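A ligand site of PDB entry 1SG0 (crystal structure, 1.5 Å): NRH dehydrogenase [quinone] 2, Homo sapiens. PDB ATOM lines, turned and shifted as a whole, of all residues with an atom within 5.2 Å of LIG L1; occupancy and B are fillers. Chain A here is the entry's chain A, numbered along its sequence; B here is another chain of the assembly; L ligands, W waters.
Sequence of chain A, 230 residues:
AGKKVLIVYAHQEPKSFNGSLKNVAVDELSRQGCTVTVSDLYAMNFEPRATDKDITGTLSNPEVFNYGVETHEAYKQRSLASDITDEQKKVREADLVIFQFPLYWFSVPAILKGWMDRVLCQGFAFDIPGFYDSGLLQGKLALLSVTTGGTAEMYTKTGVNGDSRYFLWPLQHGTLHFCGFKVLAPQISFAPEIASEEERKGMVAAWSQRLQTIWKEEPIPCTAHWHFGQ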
ATOM      1  N   HIS A  11     -10.488  20.737  19.269  1.00  0.00           N
ATOM      2  CA  HIS A  11     -11.203  19.556  18.811  1.00  0.00           C
ATOM      3  C   HIS A  11     -10.752  19.280  17.386  1.00  0.00           C
ATOM      4  O   HIS A  11     -10.555  20.195  16.601  1.00  0.00           O
ATOM      5  CB  HIS A  11     -12.722  19.714  18.876  1.00  0.00           C
ATOM      6  CG  HIS A  11     -13.453  18.407  18.883  1.00  0.00           C
ATOM      7  ND1 HIS A  11     -13.496  17.566  17.800  1.00  0.00           N
ATOM      8  CD2 HIS A  11     -14.125  17.773  19.878  1.00  0.00           C
ATOM      9  CE1 HIS A  11     -14.174  16.473  18.113  1.00  0.00           C
ATOM     10  NE2 HIS A  11     -14.566  16.576  19.369  1.00  0.00           N
ATOM     11  N   LYS A  15     -17.203  19.149  12.482  1.00  0.00           N
ATOM     12  CA  LYS A  15     -18.614  18.783  12.615  1.00  0.00           C
ATOM     13  C   LYS A  15     -19.004  18.314  14.023  1.00  0.00           C
ATOM     14  O   LYS A  15     -20.165  17.954  14.265  1.00  0.00           O
ATOM     15  CB  LYS A  15     -18.957  17.668  11.622  1.00  0.00           C
ATOM     16  CG  LYS A  15     -18.734  18.030  10.159  1.00  0.00           C
ATOM     17  CD  LYS A  15     -18.958  16.813   9.271  1.00  0.00           C
ATOM     18  CE  LYS A  15     -18.642  17.115   7.819  1.00  0.00           C
ATOM     19  NZ  LYS A  15     -18.710  15.867   6.993  1.00  0.00           N
ATOM     20  N   SER A  16     -18.046  18.320  14.935  1.00  0.00           N
ATOM     21  CA  SER A  16     -18.316  17.877  16.302  1.00  0.00           C
ATOM     22  C   SER A  16     -19.184  18.829  17.098  1.00  0.00           C
ATOM     23  O   SER A  16     -19.438  19.965  16.685  1.00  0.00           O
ATOM     24  CB  SER A  16     -16.988  17.692  17.047  1.00  0.00           C
ATOM     25  OG  SER A  16     -16.362  18.943  17.265  1.00  0.00           O
ATOM     26  N   PHE A  17     -19.641  18.364  18.260  1.00  0.00           N
ATOM     27  CA  PHE A  17     -20.470  19.193  19.125  1.00  0.00           C
ATOM     28  C   PHE A  17     -19.615  20.387  19.541  1.00  0.00           C
ATOM     29  O   PHE A  17     -20.102  21.507  19.621  1.00  0.00           O
ATOM     30  CB  PHE A  17     -20.901  18.400  20.361  1.00  0.00           C
ATOM     31  CG  PHE A  17     -22.015  19.046  21.130  1.00  0.00           C
ATOM     32  CD1 PHE A  17     -23.305  19.079  20.614  1.00  0.00           C
ATOM     33  CD2 PHE A  17     -21.770  19.634  22.376  1.00  0.00           C
ATOM     34  CE1 PHE A  17     -24.338  19.686  21.320  1.00  0.00           C
ATOM     35  CE2 PHE A  17     -22.805  20.244  23.091  1.00  0.00           C
ATOM     36  CZ  PHE A  17     -24.090  20.271  22.556  1.00  0.00           C
ATOM     37  N   ASN A  18     -18.338  20.133  19.818  1.00  0.00           N
ATOM     38  CA  ASN A  18     -17.433  21.212  20.196  1.00  0.00           C
ATOM     39  C   ASN A  18     -17.312  22.202  19.054  1.00  0.00           C
ATOM     40  O   ASN A  18     -17.302  23.412  19.272  1.00  0.00           O
ATOM     41  CB  ASN A  18     -16.049  20.653  20.529  1.00  0.00           C
ATOM     42  CG  ASN A  18     -15.902  20.329  21.993  1.00  0.00           C
ATOM     43  OD1 ASN A  18     -15.456  21.163  22.776  1.00  0.00           O
ATOM     44  ND2 ASN A  18     -16.304  19.125  22.381  1.00  0.00           N
ATOM     45  N   SER A  20     -19.495  22.865  16.837  1.00  0.00           N
ATOM     46  CA  SER A  20     -20.739  23.638  16.788  1.00  0.00           C
ATOM     47  C   SER A  20     -20.774  24.704  17.879  1.00  0.00           C
ATOM     48  O   SER A  20     -21.236  25.826  17.631  1.00  0.00           O
ATOM     49  CB  SER A  20     -21.945  22.701  16.945  1.00  0.00           C
ATOM     50  OG  SER A  20     -22.067  21.869  15.806  1.00  0.00           O
ATOM     51  N   PRO A 102     -13.324  19.310  24.770  1.00  0.00           N
ATOM     52  CA  PRO A 102     -13.973  18.130  25.321  1.00  0.00           C
ATOM     53  C   PRO A 102     -13.124  17.741  26.528  1.00  0.00           C
ATOM     54  O   PRO A 102     -11.889  17.852  26.479  1.00  0.00           O
ATOM     55  CB  PRO A 102     -13.858  17.108  24.206  1.00  0.00           C
ATOM     56  CG  PRO A 102     -12.537  17.458  23.578  1.00  0.00           C
ATOM     57  CD  PRO A 102     -12.599  18.972  23.523  1.00  0.00           C
ATOM     58  N   LEU A 103     -13.764  17.313  27.598  1.00  0.00           N
ATOM     59  CA  LEU A 103     -13.011  16.922  28.780  1.00  0.00           C
ATOM     60  C   LEU A 103     -12.203  15.666  28.471  1.00  0.00           C
ATOM     61  O   LEU A 103     -12.751  14.682  27.987  1.00  0.00           O
ATOM     62  CB  LEU A 103     -13.969  16.653  29.933  1.00  0.00           C
ATOM     63  CG  LEU A 103     -13.378  16.521  31.338  1.00  0.00           C
ATOM     64  CD1 LEU A 103     -12.841  17.842  31.825  1.00  0.00           C
ATOM     65  CD2 LEU A 103     -14.473  16.027  32.286  1.00  0.00           C
ATOM     66  N   TYR A 104     -10.898  15.713  28.729  1.00  0.00           N
ATOM     67  CA  TYR A 104     -10.014  14.567  28.536  1.00  0.00           C
ATOM     68  C   TYR A 104      -9.378  14.274  29.895  1.00  0.00           C
ATOM     69  O   TYR A 104      -8.587  15.078  30.390  1.00  0.00           O
ATOM     70  CB  TYR A 104      -8.890  14.871  27.535  1.00  0.00           C
ATOM     71  CG  TYR A 104      -9.164  14.606  26.076  1.00  0.00           C
ATOM     72  CD1 TYR A 104     -10.468  14.590  25.561  1.00  0.00           C
ATOM     73  CD2 TYR A 104      -8.105  14.451  25.176  1.00  0.00           C
ATOM     74  CE1 TYR A 104     -10.696  14.427  24.190  1.00  0.00           C
ATOM     75  CE2 TYR A 104      -8.323  14.289  23.819  1.00  0.00           C
ATOM     76  CZ  TYR A 104      -9.610  14.283  23.327  1.00  0.00           C
ATOM     77  OH  TYR A 104      -9.812  14.117  21.964  1.00  0.00           O
ATOM     78  N   TRP A 105      -9.727  13.139  30.480  1.00  0.00           N
ATOM     79  CA  TRP A 105      -9.186  12.743  31.769  1.00  0.00           C
ATOM     80  C   TRP A 105      -9.337  13.834  32.832  1.00  0.00           C
ATOM     81  O   TRP A 105      -8.370  14.234  33.487  1.00  0.00           O
ATOM     82  CB  TRP A 105      -7.722  12.311  31.600  1.00  0.00           C
ATOM     83  CG  TRP A 105      -7.568  11.028  30.812  1.00  0.00           C
ATOM     84  CD1 TRP A 105      -6.778  10.830  29.702  1.00  0.00           C
ATOM     85  CD2 TRP A 105      -8.181   9.764  31.086  1.00  0.00           C
ATOM     86  NE1 TRP A 105      -6.871   9.524  29.275  1.00  0.00           N
ATOM     87  CE2 TRP A 105      -7.731   8.852  30.113  1.00  0.00           C
ATOM     88  CE3 TRP A 105      -9.079   9.322  32.070  1.00  0.00           C
ATOM     89  CZ2 TRP A 105      -8.136   7.509  30.089  1.00  0.00           C
ATOM     90  CZ3 TRP A 105      -9.490   7.987  32.042  1.00  0.00           C
ATOM     91  CH2 TRP A 105      -9.018   7.096  31.057  1.00  0.00           C
ATOM     92  N   PHE A 106     -10.571  14.308  32.996  1.00  0.00           N
ATOM     93  CA  PHE A 106     -10.892  15.347  33.986  1.00  0.00           C
ATOM     94  C   PHE A 106     -10.077  16.619  33.785  1.00  0.00           C
ATOM     95  O   PHE A 106      -9.860  17.384  34.733  1.00  0.00           O
ATOM     96  CB  PHE A 106     -10.632  14.820  35.412  1.00  0.00           C
ATOM     97  CG  PHE A 106     -11.773  14.006  35.991  1.00  0.00           C
ATOM     98  CD1 PHE A 106     -12.586  13.217  35.184  1.00  0.00           C
ATOM     99  CD2 PHE A 106     -12.006  14.018  37.371  1.00  0.00           C
ATOM    100  CE1 PHE A 106     -13.607  12.442  35.750  1.00  0.00           C
ATOM    101  CE2 PHE A 106     -13.016  13.247  37.929  1.00  0.00           C
ATOM    102  CZ  PHE A 106     -13.815  12.456  37.125  1.00  0.00           C
ATOM    103  N   THR A 147     -17.258  20.010  27.294  1.00  0.00           N
ATOM    104  CA  THR A 147     -18.236  18.977  26.980  1.00  0.00           C
ATOM    105  C   THR A 147     -17.708  17.720  27.664  1.00  0.00           C
ATOM    106  O   THR A 147     -16.498  17.546  27.823  1.00  0.00           O
ATOM    107  CB  THR A 147     -18.377  18.737  25.462  1.00  0.00           C
ATOM    108  OG1 THR A 147     -17.135  18.257  24.925  1.00  0.00           O
ATOM    109  CG2 THR A 147     -18.767  20.026  24.751  1.00  0.00           C
ATOM    110  N   THR A 148     -18.607  16.838  28.080  1.00  0.00           N
ATOM    111  CA  THR A 148     -18.190  15.631  28.783  1.00  0.00           C
ATOM    112  C   THR A 148     -18.793  14.354  28.212  1.00  0.00           C
ATOM    113  O   THR A 148     -19.738  14.391  27.420  1.00  0.00           O
ATOM    114  CB  THR A 148     -18.607  15.688  30.251  1.00  0.00           C
ATOM    115  OG1 THR A 148     -20.039  15.555  30.352  1.00  0.00           O
ATOM    116  CG2 THR A 148     -18.182  17.000  30.883  1.00  0.00           C
ATOM    117  N   GLY A 149     -18.224  13.228  28.619  1.00  0.00           N
ATOM    118  CA  GLY A 149     -18.735  11.936  28.206  1.00  0.00           C
ATOM    119  C   GLY A 149     -19.714  11.529  29.298  1.00  0.00           C
ATOM    120  O   GLY A 149     -20.790  10.983  29.015  1.00  0.00           O
ATOM    121  N   GLY A 150     -19.356  11.827  30.543  1.00  0.00           N
ATOM    122  CA  GLY A 150     -20.203  11.492  31.670  1.00  0.00           C
ATOM    123  C   GLY A 150     -21.413  12.393  31.808  1.00  0.00           C
ATOM    124  O   GLY A 150     -21.388  13.555  31.397  1.00  0.00           O
ATOM    125  N   TYR A 155     -21.602  13.414  37.616  1.00  0.00           N
ATOM    126  CA  TYR A 155     -20.801  14.507  38.146  1.00  0.00           C
ATOM    127  C   TYR A 155     -21.457  15.196  39.336  1.00  0.00           C
ATOM    128  O   TYR A 155     -21.616  16.413  39.356  1.00  0.00           O
ATOM    129  CB  TYR A 155     -20.497  15.517  37.025  1.00  0.00           C
ATOM    130  CG  TYR A 155     -19.391  15.043  36.105  1.00  0.00           C
ATOM    131  CD1 TYR A 155     -18.065  15.017  36.531  1.00  0.00           C
ATOM    132  CD2 TYR A 155     -19.684  14.573  34.821  1.00  0.00           C
ATOM    133  CE1 TYR A 155     -17.058  14.539  35.693  1.00  0.00           C
ATOM    134  CE2 TYR A 155     -18.677  14.095  33.984  1.00  0.00           C
ATOM    135  CZ  TYR A 155     -17.364  14.069  34.428  1.00  0.00           C
ATOM    136  OH  TYR A 155     -16.359  13.591  33.622  1.00  0.00           O
ATOM    137  N   ASN A 161     -18.211  10.190  39.412  1.00  0.00           N
ATOM    138  CA  ASN A 161     -17.183  11.133  38.990  1.00  0.00           C
ATOM    139  C   ASN A 161     -16.961  12.298  39.936  1.00  0.00           C
ATOM    140  O   ASN A 161     -15.978  13.030  39.793  1.00  0.00           O
ATOM    141  CB  ASN A 161     -17.508  11.697  37.600  1.00  0.00           C
ATOM    142  CG  ASN A 161     -17.436  10.647  36.515  1.00  0.00           C
ATOM    143  OD1 ASN A 161     -16.769   9.623  36.668  1.00  0.00           O
ATOM    144  ND2 ASN A 161     -18.105  10.903  35.396  1.00  0.00           N
ATOM    145  N   PRO A 192     -23.194  15.102  25.442  1.00  0.00           N
ATOM    146  CA  PRO A 192     -23.951  15.365  24.222  1.00  0.00           C
ATOM    147  C   PRO A 192     -24.147  14.091  23.392  1.00  0.00           C
ATOM    148  O   PRO A 192     -25.117  13.972  22.641  1.00  0.00           O
ATOM    149  CB  PRO A 192     -23.118  16.423  23.508  1.00  0.00           C
ATOM    150  CG  PRO A 192     -21.718  16.108  23.966  1.00  0.00           C
ATOM    151  CD  PRO A 192     -21.916  15.847  25.438  1.00  0.00           C
ATOM    152  N   GLU A 193     -23.229  13.148  23.534  1.00  0.00           N
ATOM    153  CA  GLU A 193     -23.306  11.892  22.784  1.00  0.00           C
ATOM    154  C   GLU A 193     -24.471  11.016  23.246  1.00  0.00           C
ATOM    155  O   GLU A 193     -25.059  10.293  22.435  1.00  0.00           O
ATOM    156  CB  GLU A 193     -21.988  11.114  22.929  1.00  0.00           C
ATOM    157  CG  GLU A 193     -20.821  11.767  22.201  1.00  0.00           C
ATOM    158  CD  GLU A 193     -19.491  11.116  22.505  1.00  0.00           C
ATOM    159  OE1 GLU A 193     -19.051  11.171  23.673  1.00  0.00           O
ATOM    160  OE2 GLU A 193     -18.872  10.545  21.581  1.00  0.00           O
ATOM    161  N   GLU A 197     -31.243  14.607  20.113  1.00  0.00           N
ATOM    162  CA  GLU A 197     -31.116  15.775  19.243  1.00  0.00           C
ATOM    163  C   GLU A 197     -31.755  17.000  19.888  1.00  0.00           C
ATOM    164  O   GLU A 197     -31.170  18.082  19.877  1.00  0.00           O
ATOM    165  CB  GLU A 197     -31.772  15.501  17.889  1.00  0.00           C
ATOM    166  CG  GLU A 197     -31.082  14.438  17.069  1.00  0.00           C
ATOM    167  CD  GLU A 197     -29.637  14.785  16.767  1.00  0.00           C
ATOM    168  OE1 GLU A 197     -29.392  15.845  16.155  1.00  0.00           O
ATOM    169  OE2 GLU A 197     -28.747  14.003  17.144  1.00  0.00           O
ATOM    170  N   ARG A 200     -29.470  18.169  22.569  1.00  0.00           N
ATOM    171  CA  ARG A 200     -28.245  18.732  22.002  1.00  0.00           C
ATOM    172  C   ARG A 200     -28.536  20.144  21.507  1.00  0.00           C
ATOM    173  O   ARG A 200     -27.780  21.076  21.803  1.00  0.00           O
ATOM    174  CB  ARG A 200     -27.747  17.867  20.844  1.00  0.00           C
ATOM    175  CG  ARG A 200     -27.356  16.461  21.235  1.00  0.00           C
ATOM    176  CD  ARG A 200     -26.979  15.630  20.023  1.00  0.00           C
ATOM    177  NE  ARG A 200     -26.723  14.240  20.373  1.00  0.00           N
ATOM    178  CZ  ARG A 200     -26.464  13.278  19.494  1.00  0.00           C
ATOM    179  NH1 ARG A 200     -26.431  13.550  18.202  1.00  0.00           N
ATOM    180  NH2 ARG A 200     -26.232  12.036  19.911  1.00  0.00           N
ATOM    181  N   LYS A 201     -29.621  20.302  20.760  1.00  0.00           N
ATOM    182  CA  LYS A 201     -30.015  21.602  20.239  1.00  0.00           C
ATOM    183  C   LYS A 201     -30.256  22.555  21.395  1.00  0.00           C
ATOM    184  O   LYS A 201     -29.971  23.748  21.314  1.00  0.00           O
ATOM    185  CB  LYS A 201     -31.283  21.490  19.395  1.00  0.00           C
ATOM    186  CG  LYS A 201     -31.108  20.720  18.090  1.00  0.00           C
ATOM    187  CD  LYS A 201     -30.116  21.420  17.172  1.00  0.00           C
ATOM    188  CE  LYS A 201     -30.046  20.728  15.826  1.00  0.00           C
ATOM    189  NZ  LYS A 201     -31.369  20.716  15.131  1.00  0.00           N
ATOM    190  N   VAL A 204     -26.840  23.764  22.824  1.00  0.00           N
ATOM    191  CA  VAL A 204     -26.179  24.744  21.958  1.00  0.00           C
ATOM    192  C   VAL A 204     -26.922  26.076  22.057  1.00  0.00           C
ATOM    193  O   VAL A 204     -26.310  27.139  22.049  1.00  0.00           O
ATOM    194  CB  VAL A 204     -26.150  24.286  20.476  1.00  0.00           C
ATOM    195  CG1 VAL A 204     -25.387  22.979  20.343  1.00  0.00           C
ATOM    196  CG2 VAL A 204     -27.562  24.132  19.942  1.00  0.00           C
ATOM    197  N   ASN B  66     -14.126  10.852  15.237  1.00  0.00           N
ATOM    198  CA  ASN B  66     -14.389  10.768  16.680  1.00  0.00           C
ATOM    199  C   ASN B  66     -13.200  10.003  17.251  1.00  0.00           C
ATOM    200  O   ASN B  66     -13.104   8.780  17.098  1.00  0.00           O
ATOM    201  CB  ASN B  66     -15.684   9.997  16.925  1.00  0.00           C
ATOM    202  CG  ASN B  66     -16.075   9.951  18.387  1.00  0.00           C
ATOM    203  OD1 ASN B  66     -15.292   9.555  19.245  1.00  0.00           O
ATOM    204  ND2 ASN B  66     -17.307  10.346  18.683  1.00  0.00           N
ATOM    205  N   TYR B  67     -12.275  10.717  17.907  1.00  0.00           N
ATOM    206  CA  TYR B  67     -11.082  10.085  18.448  1.00  0.00           C
ATOM    207  C   TYR B  67     -11.339   8.856  19.325  1.00  0.00           C
ATOM    208  O   TYR B  67     -10.697   7.820  19.141  1.00  0.00           O
ATOM    209  CB  TYR B  67     -10.268  11.110  19.250  1.00  0.00           C
ATOM    210  CG  TYR B  67      -8.883  10.600  19.601  1.00  0.00           C
ATOM    211  CD1 TYR B  67      -7.854  10.573  18.654  1.00  0.00           C
ATOM    212  CD2 TYR B  67      -8.613  10.101  20.882  1.00  0.00           C
ATOM    213  CE1 TYR B  67      -6.592  10.065  18.972  1.00  0.00           C
ATOM    214  CE2 TYR B  67      -7.354   9.580  21.203  1.00  0.00           C
ATOM    215  CZ  TYR B  67      -6.357   9.563  20.244  1.00  0.00           C
ATOM    216  OH  TYR B  67      -5.120   9.021  20.555  1.00  0.00           O
ATOM    217  N   GLY B  68     -12.260   8.973  20.273  1.00  0.00           N
ATOM    218  CA  GLY B  68     -12.561   7.856  21.146  1.00  0.00           C
ATOM    219  C   GLY B  68     -13.021   6.615  20.387  1.00  0.00           C
ATOM    220  O   GLY B  68     -12.498   5.514  20.590  1.00  0.00           O
ATOM    221  N   ASP B 117      -3.718  10.677  27.534  1.00  0.00           N
ATOM    222  CA  ASP B 117      -4.774  10.777  26.521  1.00  0.00           C
ATOM    223  C   ASP B 117      -4.712   9.689  25.455  1.00  0.00           C
ATOM    224  O   ASP B 117      -5.734   9.127  25.061  1.00  0.00           O
ATOM    225  CB  ASP B 117      -4.705  12.119  25.766  1.00  0.00           C
ATOM    226  CG  ASP B 117      -4.952  13.318  26.652  1.00  0.00           C
ATOM    227  OD1 ASP B 117      -5.414  13.150  27.809  1.00  0.00           O
ATOM    228  OD2 ASP B 117      -4.705  14.452  26.158  1.00  0.00           O
ATOM    229  N   GLY B 174      -9.995  10.632  38.330  1.00  0.00           N
ATOM    230  CA  GLY B 174     -10.489  10.696  36.971  1.00  0.00           C
ATOM    231  C   GLY B 174      -9.726   9.848  35.976  1.00  0.00           C
ATOM    232  O   GLY B 174     -10.294   9.415  34.974  1.00  0.00           O
HETATM  233  P1  LIG L   1     -19.424  14.585  19.206  1.00  0.00           P
HETATM  234  O1  LIG L   1     -19.241  13.449  20.095  1.00  0.00           O
HETATM  235  O2  LIG L   1     -18.516  15.551  18.572  1.00  0.00           O
HETATM  236  O3  LIG L   1     -20.884  15.268  19.342  1.00  0.00           O
HETATM  237  C1  LIG L   1     -21.985  14.551  19.925  1.00  0.00           C
HETATM  238  C2  LIG L   1     -23.069  14.566  18.994  1.00  0.00           C
HETATM  239  O4  LIG L   1     -23.441  15.919  18.765  1.00  0.00           O
HETATM  240  C3  LIG L   1     -22.759  13.955  17.602  1.00  0.00           C
HETATM  241  O5  LIG L   1     -23.623  12.886  17.264  1.00  0.00           O
HETATM  242  C4  LIG L   1     -22.873  15.151  16.680  1.00  0.00           C
HETATM  243  O6  LIG L   1     -23.197  14.881  15.338  1.00  0.00           O
HETATM  244  C5  LIG L   1     -23.892  16.024  17.427  1.00  0.00           C
HETATM  245  N1  LIG L   1     -23.886  17.447  17.061  1.00  0.00           N
HETATM  246  C6  LIG L   1     -22.834  18.191  16.577  1.00  0.00           C
HETATM  247  N2  LIG L   1     -23.162  19.451  16.334  1.00  0.00           N
HETATM  248  C7  LIG L   1     -24.491  19.536  16.676  1.00  0.00           C
HETATM  249  C8  LIG L   1     -25.414  20.614  16.653  1.00  0.00           C
HETATM  250  N3  LIG L   1     -25.095  21.831  16.250  1.00  0.00           N
HETATM  251  N4  LIG L   1     -26.707  20.356  17.077  1.00  0.00           N
HETATM  252  C9  LIG L   1     -27.058  19.097  17.495  1.00  0.00           C
HETATM  253  N5  LIG L   1     -26.225  18.023  17.547  1.00  0.00           N
HETATM  254  C10 LIG L   1     -24.956  18.296  17.133  1.00  0.00           C
HETATM  255  N6  LIG L   1     -15.496  12.313  29.408  1.00  0.00           N
HETATM  256  C11 LIG L   1     -15.679  12.566  30.749  1.00  0.00           C
HETATM  257  O7  LIG L   1     -16.789  12.785  31.207  1.00  0.00           O
HETATM  258  N7  LIG L   1     -14.559  12.559  31.589  1.00  0.00           N
HETATM  259  C12 LIG L   1     -13.259  12.316  31.158  1.00  0.00           C
HETATM  260  O8  LIG L   1     -12.302  12.332  31.958  1.00  0.00           O
HETATM  261  C13 LIG L   1     -13.074  12.046  29.779  1.00  0.00           C
HETATM  262  N8  LIG L   1     -11.811  11.791  29.266  1.00  0.00           N
HETATM  263  C14 LIG L   1     -11.625  11.535  27.915  1.00  0.00           C
HETATM  264  C15 LIG L   1     -10.348  11.278  27.406  1.00  0.00           C
HETATM  265  C16 LIG L   1     -10.104  11.028  26.037  1.00  0.00           C
HETATM  266  C17 LIG L   1      -8.699  10.761  25.566  1.00  0.00           C
HETATM  267  C18 LIG L   1     -11.231  11.030  25.143  1.00  0.00           C
HETATM  268  C19 LIG L   1     -11.059  10.767  23.662  1.00  0.00           C
HETATM  269  C20 LIG L   1     -12.530  11.285  25.625  1.00  0.00           C
HETATM  270  C21 LIG L   1     -12.771  11.547  27.013  1.00  0.00           C
HETATM  271  N9  LIG L   1     -14.071  11.817  27.555  1.00  0.00           N
HETATM  272  C22 LIG L   1     -14.227  12.065  28.927  1.00  0.00           C
HETATM  273  C23 LIG L   1     -15.325  11.855  26.702  1.00  0.00           C
HETATM  274  C24 LIG L   1     -15.284  13.077  25.771  1.00  0.00           C
HETATM  275  O9  LIG L   1     -15.412  14.239  26.571  1.00  0.00           O
HETATM  276  C25 LIG L   1     -16.409  12.986  24.711  1.00  0.00           C
HETATM  277  O10 LIG L   1     -16.259  11.811  23.932  1.00  0.00           O
HETATM  278  C26 LIG L   1     -16.434  14.136  23.676  1.00  0.00           C
HETATM  279  O11 LIG L   1     -17.130  15.241  24.212  1.00  0.00           O
HETATM  280  C27 LIG L   1     -17.108  13.648  22.340  1.00  0.00           C
HETATM  281  O12 LIG L   1     -17.083  14.709  21.345  1.00  0.00           O
HETATM  282  P2  LIG L   1     -17.838  16.075  21.452  1.00  0.00           P
HETATM  283  O13 LIG L   1     -17.654  16.978  20.311  1.00  0.00           O
HETATM  284  O14 LIG L   1     -18.959  16.208  22.450  1.00  0.00           O
HETATM  285  O15 LIG L   1     -19.078  15.345  20.653  1.00  0.00           O
HETATM  286  C1  LG2 L   2     -13.833   9.333  33.409  1.00  0.00           C
HETATM  287  C2  LG2 L   2     -15.244   9.489  33.611  1.00  0.00           C
HETATM  288  C3  LG2 L   2     -16.152   9.272  32.518  1.00  0.00           C
HETATM  289  C4  LG2 L   2     -15.659   8.914  31.216  1.00  0.00           C
HETATM  290  C5  LG2 L   2     -14.250   8.763  31.001  1.00  0.00           C
HETATM  291  C6  LG2 L   2     -13.331   8.965  32.101  1.00  0.00           C
HETATM  292  C7  LG2 L   2     -13.779   8.422  29.655  1.00  0.00           C
HETATM  293  C8  LG2 L   2     -12.422   8.212  29.369  1.00  0.00           C
HETATM  294  C9  LG2 L   2     -11.927   7.904  28.031  1.00  0.00           C
HETATM  295  C10 LG2 L   2     -12.805   7.803  26.889  1.00  0.00           C
HETATM  296  C11 LG2 L   2     -12.258   7.507  25.582  1.00  0.00           C
HETATM  297  C12 LG2 L   2     -10.837   7.319  25.436  1.00  0.00           C
HETATM  298  C13 LG2 L   2      -9.986   7.424  26.569  1.00  0.00           C
HETATM  299  C14 LG2 L   2     -10.528   7.714  27.857  1.00  0.00           C
HETATM  300  O1  LG2 L   2     -10.304   7.055  24.213  1.00  0.00           O
HETATM  301  O2  LG2 L   2     -17.494   9.418  32.709  1.00  0.00           O
HETATM  302  O3  LG2 L   2     -12.993   9.530  34.425  1.00  0.00           O
HETATM  303  O   HOH W   1     -23.935  24.282  14.543  1.00  0.00           O
HETATM  304  O   HOH W   2     -15.929  13.072  18.989  1.00  0.00           O
HETATM  305  O   HOH W   3     -16.227  14.209  16.495  1.00  0.00           O
HETATM  306  O   HOH W   4     -13.887  14.092  21.770  1.00  0.00           O
HETATM  307  O   HOH W   5     -20.643  15.349  14.303  1.00  0.00           O
HETATM  308  O   HOH W   6     -14.515  10.119  23.110  1.00  0.00           O
HETATM  309  O   HOH W   7     -18.863  14.335  16.012  1.00  0.00           O
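The side-chain hydroxyl (OG) of Ser 20 is in hydrogen-bond range of the backbone carbonyl oxygen (O) of Ser 16, 3.4 Å away.
The backbone carbonyl oxygen of Gly 150 lies within hydrogen-bond range of the side-chain hydroxyl of Thr 148, at 2.6 Å.
The side-chain carboxylate (OE2) of Glu 193 sits at hydrogen-bond distance from the side-chain amide nitrogen (ND2) of Asn 66 of chain B (3.3 Å).
NE of Arg 200 lies within hydrogen-bond range of O of Pro 192, 2.8 Å away.
NH1 of Arg 200 is in salt-bridge range of OE2 of Glu 197, 2.6 Å away.
A ring nitrogen (ND1) of His 11 is in hydrogen-bond range of the side-chain hydroxyl (OG) of Ser 16 (3.2 Å).
The backbone NH (N) of Asn 18 sits close to the side-chain hydroxyl (OG) of Ser 16, at 3.4 Å.
N of Leu 103 sits at hydrogen-bond distance from O of Thr 147, at 2.8 Å.
The side-chain hydroxyl of Tyr 155 is in hydrogen-bond range of an oxygen (O7) of LIG L1, at 2.6 Å.
The side-chain hydroxyl (OG) of Ser 20 is in hydrogen-bond range of a nitrogen (N2) of LIG L1, 2.7 Å away.
The backbone NH (N) of Trp 105 is in hydrogen-bond range of a nitrogen (N8) of LIG L1.
The backbone NH of Gly 150 lies within hydrogen-bond range of an oxygen (O7) of LIG L1, at 2.8 Å.
O8 of LIG L1 sits at hydrogen-bond distance from N of Phe 106 (2.8 Å).
OE1 of Glu 193 is in hydrogen-bond range of O10 of LIG L1 (2.9 Å).
The backbone NH (N) of Gly 149 is in hydrogen-bond range of a nitrogen (N6) of LIG L1 (3.0 Å).
An oxygen (O5) of LIG L1 sits at hydrogen-bond distance from the guanidinium group (NH1) of Arg 200 (3.0 Å).
N of Phe 17 lies within hydrogen-bond range of O2 of LIG L1, at 3.0 Å.
O9 of LIG L1 is in hydrogen-bond range of O of Leu 103 (3.0 Å).
The side-chain hydroxyl (OG1) of Thr 147 sits at hydrogen-bond distance from an oxygen (O11) of LIG L1, 3.1 Å away.
A ring nitrogen (NE2) of His 11 is in hydrogen-bond range of an oxygen (O13) of LIG L1 (3.3 Å).
The backbone NH of Asn 18 is in hydrogen-bond range of an oxygen (O13) of LIG L1 (3.3 Å).
An oxygen (O13) of LIG L1 sits at hydrogen-bond distance from the side-chain amide nitrogen (ND2) of Asn 18.
O of Gly 174 of chain B sits at hydrogen-bond distance from O3 of LG2 L2 (2.8 Å).
An oxygen (O2) of LG2 L2 sits at hydrogen-bond distance from the side-chain amide nitrogen (ND2) of Asn 161 (3.1 Å).
O of Lys 15 touches C6 of LIG L1, at 3.5 Å.
Ser 16 touches LIG L1.
Pro 102 touches LIG L1.
Tyr 104 touches LIG L1.
CB of Thr 148 touches O7 of LIG L1 (3.6 Å).
CG of Pro 192 touches O14 of LIG L1 (3.1 Å).
Lys 201 touches LIG L1 (CD to N4, 3.6 Å).
Asn 66 of chain B touches LIG L1 (ND2 to O1, 3.9 Å).
CD2 of Tyr 67 of chain B touches C19 of LIG L1, at 3.8 Å.
Asp 117 of chain B touches LIG L1 (O to C17, 3.4 Å).
Hydrophobic or aromatic side chains within 4 Å of LIG L1: His 11, Phe 17, Pro 102, Leu 103, Tyr 104, Phe 106, Tyr 155, Pro 192 and Tyr 67 of chain B.
Water W5 lies within hydrogen-bond range of the backbone carbonyl oxygen (O) of Lys 15 and an oxygen (O6) of LIG L1.
Water W2 bridges the side-chain amide nitrogen (ND2) of Asn 66 of chain B and an oxygen (O12) of LIG L1.
Water W1 bridges a nitrogen (N3) of LIG L1 (3.2 Å) and the side-chain hydroxyl of Ser 20 (3.3 Å).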
